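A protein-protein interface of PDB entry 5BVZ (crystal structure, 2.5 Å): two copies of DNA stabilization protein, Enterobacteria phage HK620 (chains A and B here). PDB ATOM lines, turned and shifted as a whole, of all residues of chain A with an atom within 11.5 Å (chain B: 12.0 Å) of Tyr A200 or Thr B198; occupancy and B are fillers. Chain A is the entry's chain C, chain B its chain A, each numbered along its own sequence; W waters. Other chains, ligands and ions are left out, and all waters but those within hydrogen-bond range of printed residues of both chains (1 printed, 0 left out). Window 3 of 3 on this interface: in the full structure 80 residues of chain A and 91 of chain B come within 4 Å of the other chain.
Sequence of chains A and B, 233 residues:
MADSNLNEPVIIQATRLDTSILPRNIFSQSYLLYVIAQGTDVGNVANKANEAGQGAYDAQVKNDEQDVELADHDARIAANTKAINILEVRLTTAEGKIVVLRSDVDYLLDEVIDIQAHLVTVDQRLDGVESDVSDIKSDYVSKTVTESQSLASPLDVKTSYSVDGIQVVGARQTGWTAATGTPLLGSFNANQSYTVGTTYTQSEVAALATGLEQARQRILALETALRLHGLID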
ATOM      1  N   THR A 195     -12.018  -6.877 -22.589  1.00  0.00           N
ATOM      2  CA  THR A 195     -13.221  -6.103 -22.888  1.00  0.00           C
ATOM      3  C   THR A 195     -12.913  -4.639 -23.184  1.00  0.00           C
ATOM      4  O   THR A 195     -12.176  -3.989 -22.443  1.00  0.00           O
ATOM      5  CB  THR A 195     -14.230  -6.162 -21.715  1.00  0.00           C
ATOM      6  OG1 THR A 195     -14.609  -7.521 -21.466  1.00  0.00           O
ATOM      7  CG2 THR A 195     -15.475  -5.340 -22.027  1.00  0.00           C
ATOM      8  N   VAL A 196     -13.470  -4.125 -24.276  1.00  0.00           N
ATOM      9  CA  VAL A 196     -13.381  -2.701 -24.583  1.00  0.00           C
ATOM     10  C   VAL A 196     -14.775  -2.130 -24.849  1.00  0.00           C
ATOM     11  O   VAL A 196     -15.415  -2.473 -25.840  1.00  0.00           O
ATOM     12  CB  VAL A 196     -12.473  -2.438 -25.798  1.00  0.00           C
ATOM     13  CG1 VAL A 196     -12.503  -0.970 -26.169  1.00  0.00           C
ATOM     14  CG2 VAL A 196     -11.044  -2.893 -25.507  1.00  0.00           C
ATOM     15  N   GLY A 197     -15.234  -1.251 -23.963  1.00  0.00           N
ATOM     16  CA  GLY A 197     -16.568  -0.680 -24.055  1.00  0.00           C
ATOM     17  C   GLY A 197     -16.670   0.552 -24.940  1.00  0.00           C
ATOM     18  O   GLY A 197     -15.672   1.034 -25.478  1.00  0.00           O
ATOM     19  N   THR A 198     -17.887   1.068 -25.087  1.00  0.00           N
ATOM     20  CA  THR A 198     -18.133   2.225 -25.942  1.00  0.00           C
ATOM     21  C   THR A 198     -17.631   3.513 -25.301  1.00  0.00           C
ATOM     22  O   THR A 198     -17.477   4.533 -25.973  1.00  0.00           O
ATOM     23  CB  THR A 198     -19.627   2.378 -26.263  1.00  0.00           C
ATOM     24  OG1 THR A 198     -20.370   2.512 -25.045  1.00  0.00           O
ATOM     25  CG2 THR A 198     -20.129   1.162 -27.033  1.00  0.00           C
ATOM     26  N   THR A 199     -17.392   3.462 -23.996  1.00  0.00           N
ATOM     27  CA  THR A 199     -16.844   4.601 -23.269  1.00  0.00           C
ATOM     28  C   THR A 199     -15.571   4.186 -22.537  1.00  0.00           C
ATOM     29  O   THR A 199     -15.413   3.023 -22.159  1.00  0.00           O
ATOM     30  CB  THR A 199     -17.850   5.181 -22.259  1.00  0.00           C
ATOM     31  OG1 THR A 199     -18.251   4.163 -21.334  1.00  0.00           O
ATOM     32  CG2 THR A 199     -19.068   5.723 -22.983  1.00  0.00           C
ATOM     33  N   TYR A 200     -14.664   5.141 -22.352  1.00  0.00           N
ATOM     34  CA  TYR A 200     -13.391   4.886 -21.691  1.00  0.00           C
ATOM     35  C   TYR A 200     -13.598   4.364 -20.275  1.00  0.00           C
ATOM     36  O   TYR A 200     -14.266   4.998 -19.459  1.00  0.00           O
ATOM     37  CB  TYR A 200     -12.545   6.158 -21.658  1.00  0.00           C
ATOM     38  CG  TYR A 200     -11.202   5.997 -20.981  1.00  0.00           C
ATOM     39  CD1 TYR A 200     -10.103   5.519 -21.683  1.00  0.00           C
ATOM     40  CD2 TYR A 200     -11.031   6.327 -19.644  1.00  0.00           C
ATOM     41  CE1 TYR A 200      -8.871   5.377 -21.073  1.00  0.00           C
ATOM     42  CE2 TYR A 200      -9.807   6.186 -19.026  1.00  0.00           C
ATOM     43  CZ  TYR A 200      -8.730   5.710 -19.742  1.00  0.00           C
ATOM     44  OH  TYR A 200      -7.509   5.574 -19.123  1.00  0.00           O
ATOM     45  N   THR A 201     -13.004   3.213 -19.988  1.00  0.00           N
ATOM     46  CA  THR A 201     -13.066   2.627 -18.658  1.00  0.00           C
ATOM     47  C   THR A 201     -11.657   2.334 -18.169  1.00  0.00           C
ATOM     48  O   THR A 201     -10.909   1.592 -18.814  1.00  0.00           O
ATOM     49  CB  THR A 201     -13.890   1.338 -18.651  1.00  0.00           C
ATOM     50  OG1 THR A 201     -15.173   1.588 -19.237  1.00  0.00           O
ATOM     51  CG2 THR A 201     -14.059   0.826 -17.231  1.00  0.00           C
ATOM     52  N   GLN A 202     -11.304   2.911 -17.026  1.00  0.00           N
ATOM     53  CA  GLN A 202      -9.942   2.827 -16.524  1.00  0.00           C
ATOM     54  C   GLN A 202      -9.497   1.376 -16.309  1.00  0.00           C
ATOM     55  O   GLN A 202      -8.413   0.993 -16.741  1.00  0.00           O
ATOM     56  CB  GLN A 202      -9.820   3.639 -15.232  1.00  0.00           C
ATOM     57  CG  GLN A 202      -8.401   3.829 -14.703  1.00  0.00           C
ATOM     58  CD  GLN A 202      -7.925   2.690 -13.826  1.00  0.00           C
ATOM     59  OE1 GLN A 202      -8.725   2.002 -13.190  1.00  0.00           O
ATOM     60  NE2 GLN A 202      -6.611   2.498 -13.772  1.00  0.00           N
ATOM     61  N   SER A 203     -10.353   0.563 -15.696  1.00  0.00           N
ATOM     62  CA  SER A 203      -9.999  -0.822 -15.380  1.00  0.00           C
ATOM     63  C   SER A 203      -9.811  -1.670 -16.639  1.00  0.00           C
ATOM     64  O   SER A 203      -8.985  -2.586 -16.668  1.00  0.00           O
ATOM     65  CB  SER A 203     -11.063  -1.459 -14.477  1.00  0.00           C
ATOM     66  OG  SER A 203     -12.323  -1.537 -15.128  1.00  0.00           O
ATOM     67  N   GLU A 204     -10.579  -1.369 -17.679  1.00  0.00           N
ATOM     68  CA  GLU A 204     -10.469  -2.097 -18.934  1.00  0.00           C
ATOM     69  C   GLU A 204      -9.149  -1.802 -19.639  1.00  0.00           C
ATOM     70  O   GLU A 204      -8.451  -2.718 -20.074  1.00  0.00           O
ATOM     71  CB  GLU A 204     -11.643  -1.767 -19.845  1.00  0.00           C
ATOM     72  CG  GLU A 204     -12.960  -2.314 -19.349  1.00  0.00           C
ATOM     73  CD  GLU A 204     -14.107  -1.961 -20.264  1.00  0.00           C
ATOM     74  OE1 GLU A 204     -15.179  -2.588 -20.140  1.00  0.00           O
ATOM     75  OE2 GLU A 204     -13.934  -1.056 -21.109  1.00  0.00           O
ATOM     76  N   VAL A 205      -8.810  -0.522 -19.756  1.00  0.00           N
ATOM     77  CA  VAL A 205      -7.557  -0.135 -20.390  1.00  0.00           C
ATOM     78  C   VAL A 205      -6.364  -0.594 -19.552  1.00  0.00           C
ATOM     79  O   VAL A 205      -5.351  -1.033 -20.096  1.00  0.00           O
ATOM     80  CB  VAL A 205      -7.492   1.401 -20.613  1.00  0.00           C
ATOM     81  CG1 VAL A 205      -6.168   1.816 -21.249  1.00  0.00           C
ATOM     82  CG2 VAL A 205      -8.675   1.865 -21.464  1.00  0.00           C
ATOM     83  N   ALA A 206      -6.509  -0.530 -18.230  1.00  0.00           N
ATOM     84  CA  ALA A 206      -5.469  -0.989 -17.309  1.00  0.00           C
ATOM     85  C   ALA A 206      -5.227  -2.491 -17.440  1.00  0.00           C
ATOM     86  O   ALA A 206      -4.087  -2.953 -17.373  1.00  0.00           O
ATOM     87  CB  ALA A 206      -5.839  -0.640 -15.880  1.00  0.00           C
ATOM     88  N   ALA A 207      -6.305  -3.244 -17.639  1.00  0.00           N
ATOM     89  CA  ALA A 207      -6.209  -4.685 -17.835  1.00  0.00           C
ATOM     90  C   ALA A 207      -5.407  -4.965 -19.094  1.00  0.00           C
ATOM     91  O   ALA A 207      -4.646  -5.934 -19.161  1.00  0.00           O
ATOM     92  CB  ALA A 207      -7.589  -5.310 -17.926  1.00  0.00           C
ATOM     93  N   LEU A 208      -5.591  -4.105 -20.093  1.00  0.00           N
ATOM     94  CA  LEU A 208      -4.813  -4.170 -21.314  1.00  0.00           C
ATOM     95  C   LEU A 208      -3.332  -3.981 -20.993  1.00  0.00           C
ATOM     96  O   LEU A 208      -2.487  -4.775 -21.426  1.00  0.00           O
ATOM     97  CB  LEU A 208      -5.296  -3.110 -22.306  1.00  0.00           C
ATOM     98  CG  LEU A 208      -5.445  -3.488 -23.774  1.00  0.00           C
ATOM     99  CD1 LEU A 208      -6.386  -4.661 -23.914  1.00  0.00           C
ATOM    100  CD2 LEU A 208      -5.976  -2.292 -24.545  1.00  0.00           C
ATOM    101  N   ALA A 209      -3.032  -2.958 -20.195  1.00  0.00           N
ATOM    102  CA  ALA A 209      -1.651  -2.663 -19.817  1.00  0.00           C
ATOM    103  C   ALA A 209      -1.008  -3.850 -19.114  1.00  0.00           C
ATOM    104  O   ALA A 209       0.138  -4.191 -19.388  1.00  0.00           O
ATOM    105  CB  ALA A 209      -1.588  -1.433 -18.938  1.00  0.00           C
ATOM    106  N   TYR B 194       3.067   0.840 -18.037  1.00  0.00           N
ATOM    107  CA  TYR B 194       2.274   1.761 -18.834  1.00  0.00           C
ATOM    108  C   TYR B 194       1.187   2.403 -17.980  1.00  0.00           C
ATOM    109  O   TYR B 194       0.278   1.720 -17.512  1.00  0.00           O
ATOM    110  CB  TYR B 194       1.669   1.013 -20.018  1.00  0.00           C
ATOM    111  CG  TYR B 194       2.723   0.335 -20.867  1.00  0.00           C
ATOM    112  CD1 TYR B 194       3.368   1.018 -21.887  1.00  0.00           C
ATOM    113  CD2 TYR B 194       3.099  -0.981 -20.618  1.00  0.00           C
ATOM    114  CE1 TYR B 194       4.339   0.405 -22.650  1.00  0.00           C
ATOM    115  CE2 TYR B 194       4.075  -1.605 -21.375  1.00  0.00           C
ATOM    116  CZ  TYR B 194       4.689  -0.909 -22.388  1.00  0.00           C
ATOM    117  OH  TYR B 194       5.657  -1.529 -23.143  1.00  0.00           O
ATOM    118  N   THR B 195       1.274   3.716 -17.787  1.00  0.00           N
ATOM    119  CA  THR B 195       0.318   4.419 -16.938  1.00  0.00           C
ATOM    120  C   THR B 195      -1.039   4.520 -17.618  1.00  0.00           C
ATOM    121  O   THR B 195      -1.138   4.863 -18.796  1.00  0.00           O
ATOM    122  CB  THR B 195       0.802   5.842 -16.559  1.00  0.00           C
ATOM    123  OG1 THR B 195       1.002   6.618 -17.747  1.00  0.00           O
ATOM    124  CG2 THR B 195       2.105   5.782 -15.778  1.00  0.00           C
ATOM    125  N   VAL B 196      -2.080   4.181 -16.870  1.00  0.00           N
ATOM    126  CA  VAL B 196      -3.452   4.345 -17.325  1.00  0.00           C
ATOM    127  C   VAL B 196      -4.232   5.140 -16.278  1.00  0.00           C
ATOM    128  O   VAL B 196      -4.455   4.666 -15.165  1.00  0.00           O
ATOM    129  CB  VAL B 196      -4.135   2.979 -17.576  1.00  0.00           C
ATOM    130  CG1 VAL B 196      -5.610   3.166 -17.907  1.00  0.00           C
ATOM    131  CG2 VAL B 196      -3.415   2.211 -18.686  1.00  0.00           C
ATOM    132  N   GLY B 197      -4.636   6.354 -16.640  1.00  0.00           N
ATOM    133  CA  GLY B 197      -5.336   7.237 -15.722  1.00  0.00           C
ATOM    134  C   GLY B 197      -6.833   7.010 -15.719  1.00  0.00           C
ATOM    135  O   GLY B 197      -7.340   6.197 -16.492  1.00  0.00           O
ATOM    136  N   THR B 198      -7.541   7.727 -14.851  1.00  0.00           N
ATOM    137  CA  THR B 198      -8.989   7.580 -14.740  1.00  0.00           C
ATOM    138  C   THR B 198      -9.712   8.262 -15.909  1.00  0.00           C
ATOM    139  O   THR B 198     -10.886   7.985 -16.167  1.00  0.00           O
ATOM    140  CB  THR B 198      -9.522   8.142 -13.399  1.00  0.00           C
ATOM    141  OG1 THR B 198      -9.176   9.526 -13.273  1.00  0.00           O
ATOM    142  CG2 THR B 198      -8.930   7.372 -12.234  1.00  0.00           C
ATOM    143  N   THR B 199      -9.011   9.147 -16.613  1.00  0.00           N
ATOM    144  CA  THR B 199      -9.580   9.791 -17.794  1.00  0.00           C
ATOM    145  C   THR B 199      -8.680   9.508 -18.997  1.00  0.00           C
ATOM    146  O   THR B 199      -7.466   9.343 -18.853  1.00  0.00           O
ATOM    147  CB  THR B 199      -9.755  11.327 -17.615  1.00  0.00           C
ATOM    148  OG1 THR B 199      -8.499  11.938 -17.293  1.00  0.00           O
ATOM    149  CG2 THR B 199     -10.766  11.634 -16.511  1.00  0.00           C
ATOM    150  N   TYR B 200      -9.290   9.432 -20.178  1.00  0.00           N
ATOM    151  CA  TYR B 200      -8.569   9.123 -21.411  1.00  0.00           C
ATOM    152  C   TYR B 200      -7.479  10.139 -21.741  1.00  0.00           C
ATOM    153  O   TYR B 200      -7.727  11.341 -21.813  1.00  0.00           O
ATOM    154  CB  TYR B 200      -9.538   9.013 -22.586  1.00  0.00           C
ATOM    155  CG  TYR B 200      -8.862   8.717 -23.909  1.00  0.00           C
ATOM    156  CD1 TYR B 200      -8.542   7.414 -24.273  1.00  0.00           C
ATOM    157  CD2 TYR B 200      -8.556   9.741 -24.799  1.00  0.00           C
ATOM    158  CE1 TYR B 200      -7.929   7.140 -25.484  1.00  0.00           C
ATOM    159  CE2 TYR B 200      -7.942   9.477 -26.012  1.00  0.00           C
ATOM    160  CZ  TYR B 200      -7.631   8.175 -26.351  1.00  0.00           C
ATOM    161  OH  TYR B 200      -7.024   7.910 -27.561  1.00  0.00           O
ATOM    162  N   THR B 201      -6.272   9.627 -21.937  1.00  0.00           N
ATOM    163  CA  THR B 201      -5.120  10.423 -22.325  1.00  0.00           C
ATOM    164  C   THR B 201      -4.473   9.804 -23.557  1.00  0.00           C
ATOM    165  O   THR B 201      -4.116   8.623 -23.540  1.00  0.00           O
ATOM    166  CB  THR B 201      -4.087  10.499 -21.194  1.00  0.00           C
ATOM    167  OG1 THR B 201      -4.721  10.955 -19.992  1.00  0.00           O
ATOM    168  CG2 THR B 201      -2.945  11.436 -21.571  1.00  0.00           C
ATOM    169  N   GLN B 202      -4.337  10.587 -24.624  1.00  0.00           N
ATOM    170  CA  GLN B 202      -3.808  10.063 -25.881  1.00  0.00           C
ATOM    171  C   GLN B 202      -2.406   9.472 -25.723  1.00  0.00           C
ATOM    172  O   GLN B 202      -2.121   8.394 -26.249  1.00  0.00           O
ATOM    173  CB  GLN B 202      -3.783  11.152 -26.957  1.00  0.00           C
ATOM    174  CG  GLN B 202      -3.390  10.630 -28.335  1.00  0.00           C
ATOM    175  CD  GLN B 202      -3.285  11.727 -29.369  1.00  0.00           C
ATOM    176  OE1 GLN B 202      -3.072  12.891 -29.033  1.00  0.00           O
ATOM    177  NE2 GLN B 202      -3.429  11.364 -30.636  1.00  0.00           N
ATOM    178  N   SER B 203      -1.543  10.175 -24.991  1.00  0.00           N
ATOM    179  CA  SER B 203      -0.147   9.765 -24.824  1.00  0.00           C
ATOM    180  C   SER B 203      -0.001   8.454 -24.044  1.00  0.00           C
ATOM    181  O   SER B 203       0.941   7.689 -24.271  1.00  0.00           O
ATOM    182  CB  SER B 203       0.656  10.870 -24.132  1.00  0.00           C
ATOM    183  OG  SER B 203       0.180  11.116 -22.823  1.00  0.00           O
ATOM    184  N   GLU B 204      -0.906   8.210 -23.103  1.00  0.00           N
ATOM    185  CA  GLU B 204      -0.870   6.964 -22.343  1.00  0.00           C
ATOM    186  C   GLU B 204      -1.268   5.773 -23.217  1.00  0.00           C
ATOM    187  O   GLU B 204      -0.555   4.768 -23.281  1.00  0.00           O
ATOM    188  CB  GLU B 204      -1.778   7.056 -21.116  1.00  0.00           C
ATOM    189  CG  GLU B 204      -1.276   8.015 -20.055  1.00  0.00           C
ATOM    190  CD  GLU B 204      -2.208   8.090 -18.858  1.00  0.00           C
ATOM    191  OE1 GLU B 204      -1.783   8.608 -17.805  1.00  0.00           O
ATOM    192  OE2 GLU B 204      -3.368   7.635 -18.973  1.00  0.00           O
ATOM    193  N   VAL B 205      -2.391   5.902 -23.916  1.00  0.00           N
ATOM    194  CA  VAL B 205      -2.865   4.836 -24.783  1.00  0.00           C
ATOM    195  C   VAL B 205      -1.902   4.621 -25.946  1.00  0.00           C
ATOM    196  O   VAL B 205      -1.689   3.489 -26.376  1.00  0.00           O
ATOM    197  CB  VAL B 205      -4.282   5.136 -25.310  1.00  0.00           C
ATOM    198  CG1 VAL B 205      -4.777   4.016 -26.216  1.00  0.00           C
ATOM    199  CG2 VAL B 205      -5.235   5.342 -24.146  1.00  0.00           C
ATOM    200  N   ALA B 206      -1.299   5.702 -26.431  1.00  0.00           N
ATOM    201  CA  ALA B 206      -0.306   5.603 -27.499  1.00  0.00           C
ATOM    202  C   ALA B 206       0.908   4.800 -27.038  1.00  0.00           C
ATOM    203  O   ALA B 206       1.483   4.027 -27.809  1.00  0.00           O
ATOM    204  CB  ALA B 206       0.123   6.986 -27.960  1.00  0.00           C
ATOM    205  N   ALA B 207       1.287   4.988 -25.777  1.00  0.00           N
ATOM    206  CA  ALA B 207       2.404   4.255 -25.187  1.00  0.00           C
ATOM    207  C   ALA B 207       2.104   2.762 -25.147  1.00  0.00           C
ATOM    208  O   ALA B 207       2.994   1.941 -25.341  1.00  0.00           O
ATOM    209  CB  ALA B 207       2.710   4.776 -23.792  1.00  0.00           C
ATOM    210  N   LEU B 208       0.846   2.423 -24.883  1.00  0.00           N
ATOM    211  CA  LEU B 208       0.394   1.039 -24.946  1.00  0.00           C
ATOM    212  C   LEU B 208       0.575   0.488 -26.340  1.00  0.00           C
ATOM    213  O   LEU B 208       1.095  -0.611 -26.520  1.00  0.00           O
ATOM    214  CB  LEU B 208      -1.074   0.915 -24.543  1.00  0.00           C
ATOM    215  CG  LEU B 208      -1.369   0.886 -23.054  1.00  0.00           C
ATOM    216  CD1 LEU B 208      -2.865   0.747 -22.839  1.00  0.00           C
ATOM    217  CD2 LEU B 208      -0.617  -0.275 -22.429  1.00  0.00           C
ATOM    218  N   ALA B 209       0.141   1.263 -27.327  1.00  0.00           N
ATOM    219  CA  ALA B 209       0.259   0.855 -28.716  1.00  0.00           C
ATOM    220  C   ALA B 209       1.717   0.595 -29.078  1.00  0.00           C
ATOM    221  O   ALA B 209       2.029  -0.428 -29.684  1.00  0.00           O
ATOM    222  CB  ALA B 209      -0.338   1.914 -29.634  1.00  0.00           C
HETATM  223  O   HOH W   1      -5.491   6.957 -20.733  1.00  0.00           O
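The backbone carbonyl oxygen (O) of Val B196 lies within hydrogen-bond range of the side-chain amide nitrogen (NE2) of Gln A202, 3.4 Å away. OH of Tyr A200 sits at hydrogen-bond distance from O of Gly B197 (2.7 Å).
Water W1 lies within hydrogen-bond range of OE2 of Glu B204, OH of Tyr A200 and N of Thr B201.
Of the 16 printed residues of chain B, 7 touch a printed residue of chain A. Hydrophobic or aromatic side chains of chain B within 4 Å of the printed part of chain A: Val B196, Tyr B200 and Leu B208. Among the printed residues, 13 pairs touch across the chains.
N of Gly B197 sits at hydrogen-bond distance from OE2 of Glu B204. The backbone carbonyl oxygen (O) of Thr B199 sits at hydrogen-bond distance from the side-chain hydroxyl (OG1) of Thr B201, at 3.4 Å.
Tyr A200 touches its own counterpart, Tyr B200. Gln A202 touches Val B196, but with the chains exchanged Val A196 does not touch Gln B202 (14.0 Å). Val A205 touches Val B196, but with the chains exchanged Val A196 does not touch Val B205 (9.2 Å). Ala A209 touches Leu B208, but with the chains exchanged Leu A208 does not touch Ala B209 (7.6 Å). Positions printed for both chains: 195, 196, 197, 198, 199, 200, 201, 202, 203, 204, 205, 206, 207, 208 and 209. Of the 13 pairs that touch across the chains among the printed residues, 1 has its exchanged pair printed and touching as well.
No residue of chain B comes within 4 Å of Gly A197. No residue of chain B comes within 4 Å of Thr A199. Of chain B, only Val B196 (3.3 Å), Gly B197 (2.7 Å), Thr B198 (3.5 Å), Thr B199 (3.5 Å) and Tyr B200 (3.5 Å) come within 4 Å of Tyr A200. Of the printed residues of chain B, Gln A202 touches Val B196 (3.4 Å), Gly B197 (3.2 Å) and Thr B198 (3.8 Å). Printed residues of chain B within 4 Å of Ala A209: Tyr B194 and Leu B208. Printed residues of chain A within 4 Å of Tyr B194: Ala A209. Of chain A, only Tyr A200, Gln A202, Val A205 and Ala A206 come within 4 Å of Val B196. Gly B197 touches just these residues of chain A: Tyr A200 (2.7 Å) and Gln A202 (3.2 Å). Of chain A, only Tyr A200 and Gln A202 come within 4 Å of Thr B198. Thr B199 touches just one residue of chain A: Tyr A200 (3.5 Å). Tyr B200 touches one residue of chain A. Val B205 touches none of the printed residues of chain A. Ala B206 touches none of the printed residues of chain A. The nearest residue of chain A that does not touch Thr B198 is Thr A201 (6.0 Å).
OH of Tyr A200 touches CG1 of Val B196, 3.3 Å away. Tyr A200 touches Thr B198 (CE2 to O, 3.5 Å). CE2 of Tyr A200 touches C of Thr B199 (3.5 Å). CE2 of Tyr A200 touches N of Tyr B200 (3.5 Å). Gln A202 touches Gly B197 (CG to O, 3.2 Å). CG of Gln A202 touches CA of Thr B198 (3.8 Å). CD1 of Leu B208 touches CG1 of Val A205 (3.8 Å). Ala A206 touches Val B196. Tyr B194 touches Ala A209 (O to CB, 3.9 Å). CA of Ala A209 touches CD2 of Leu B208 (3.7 Å).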
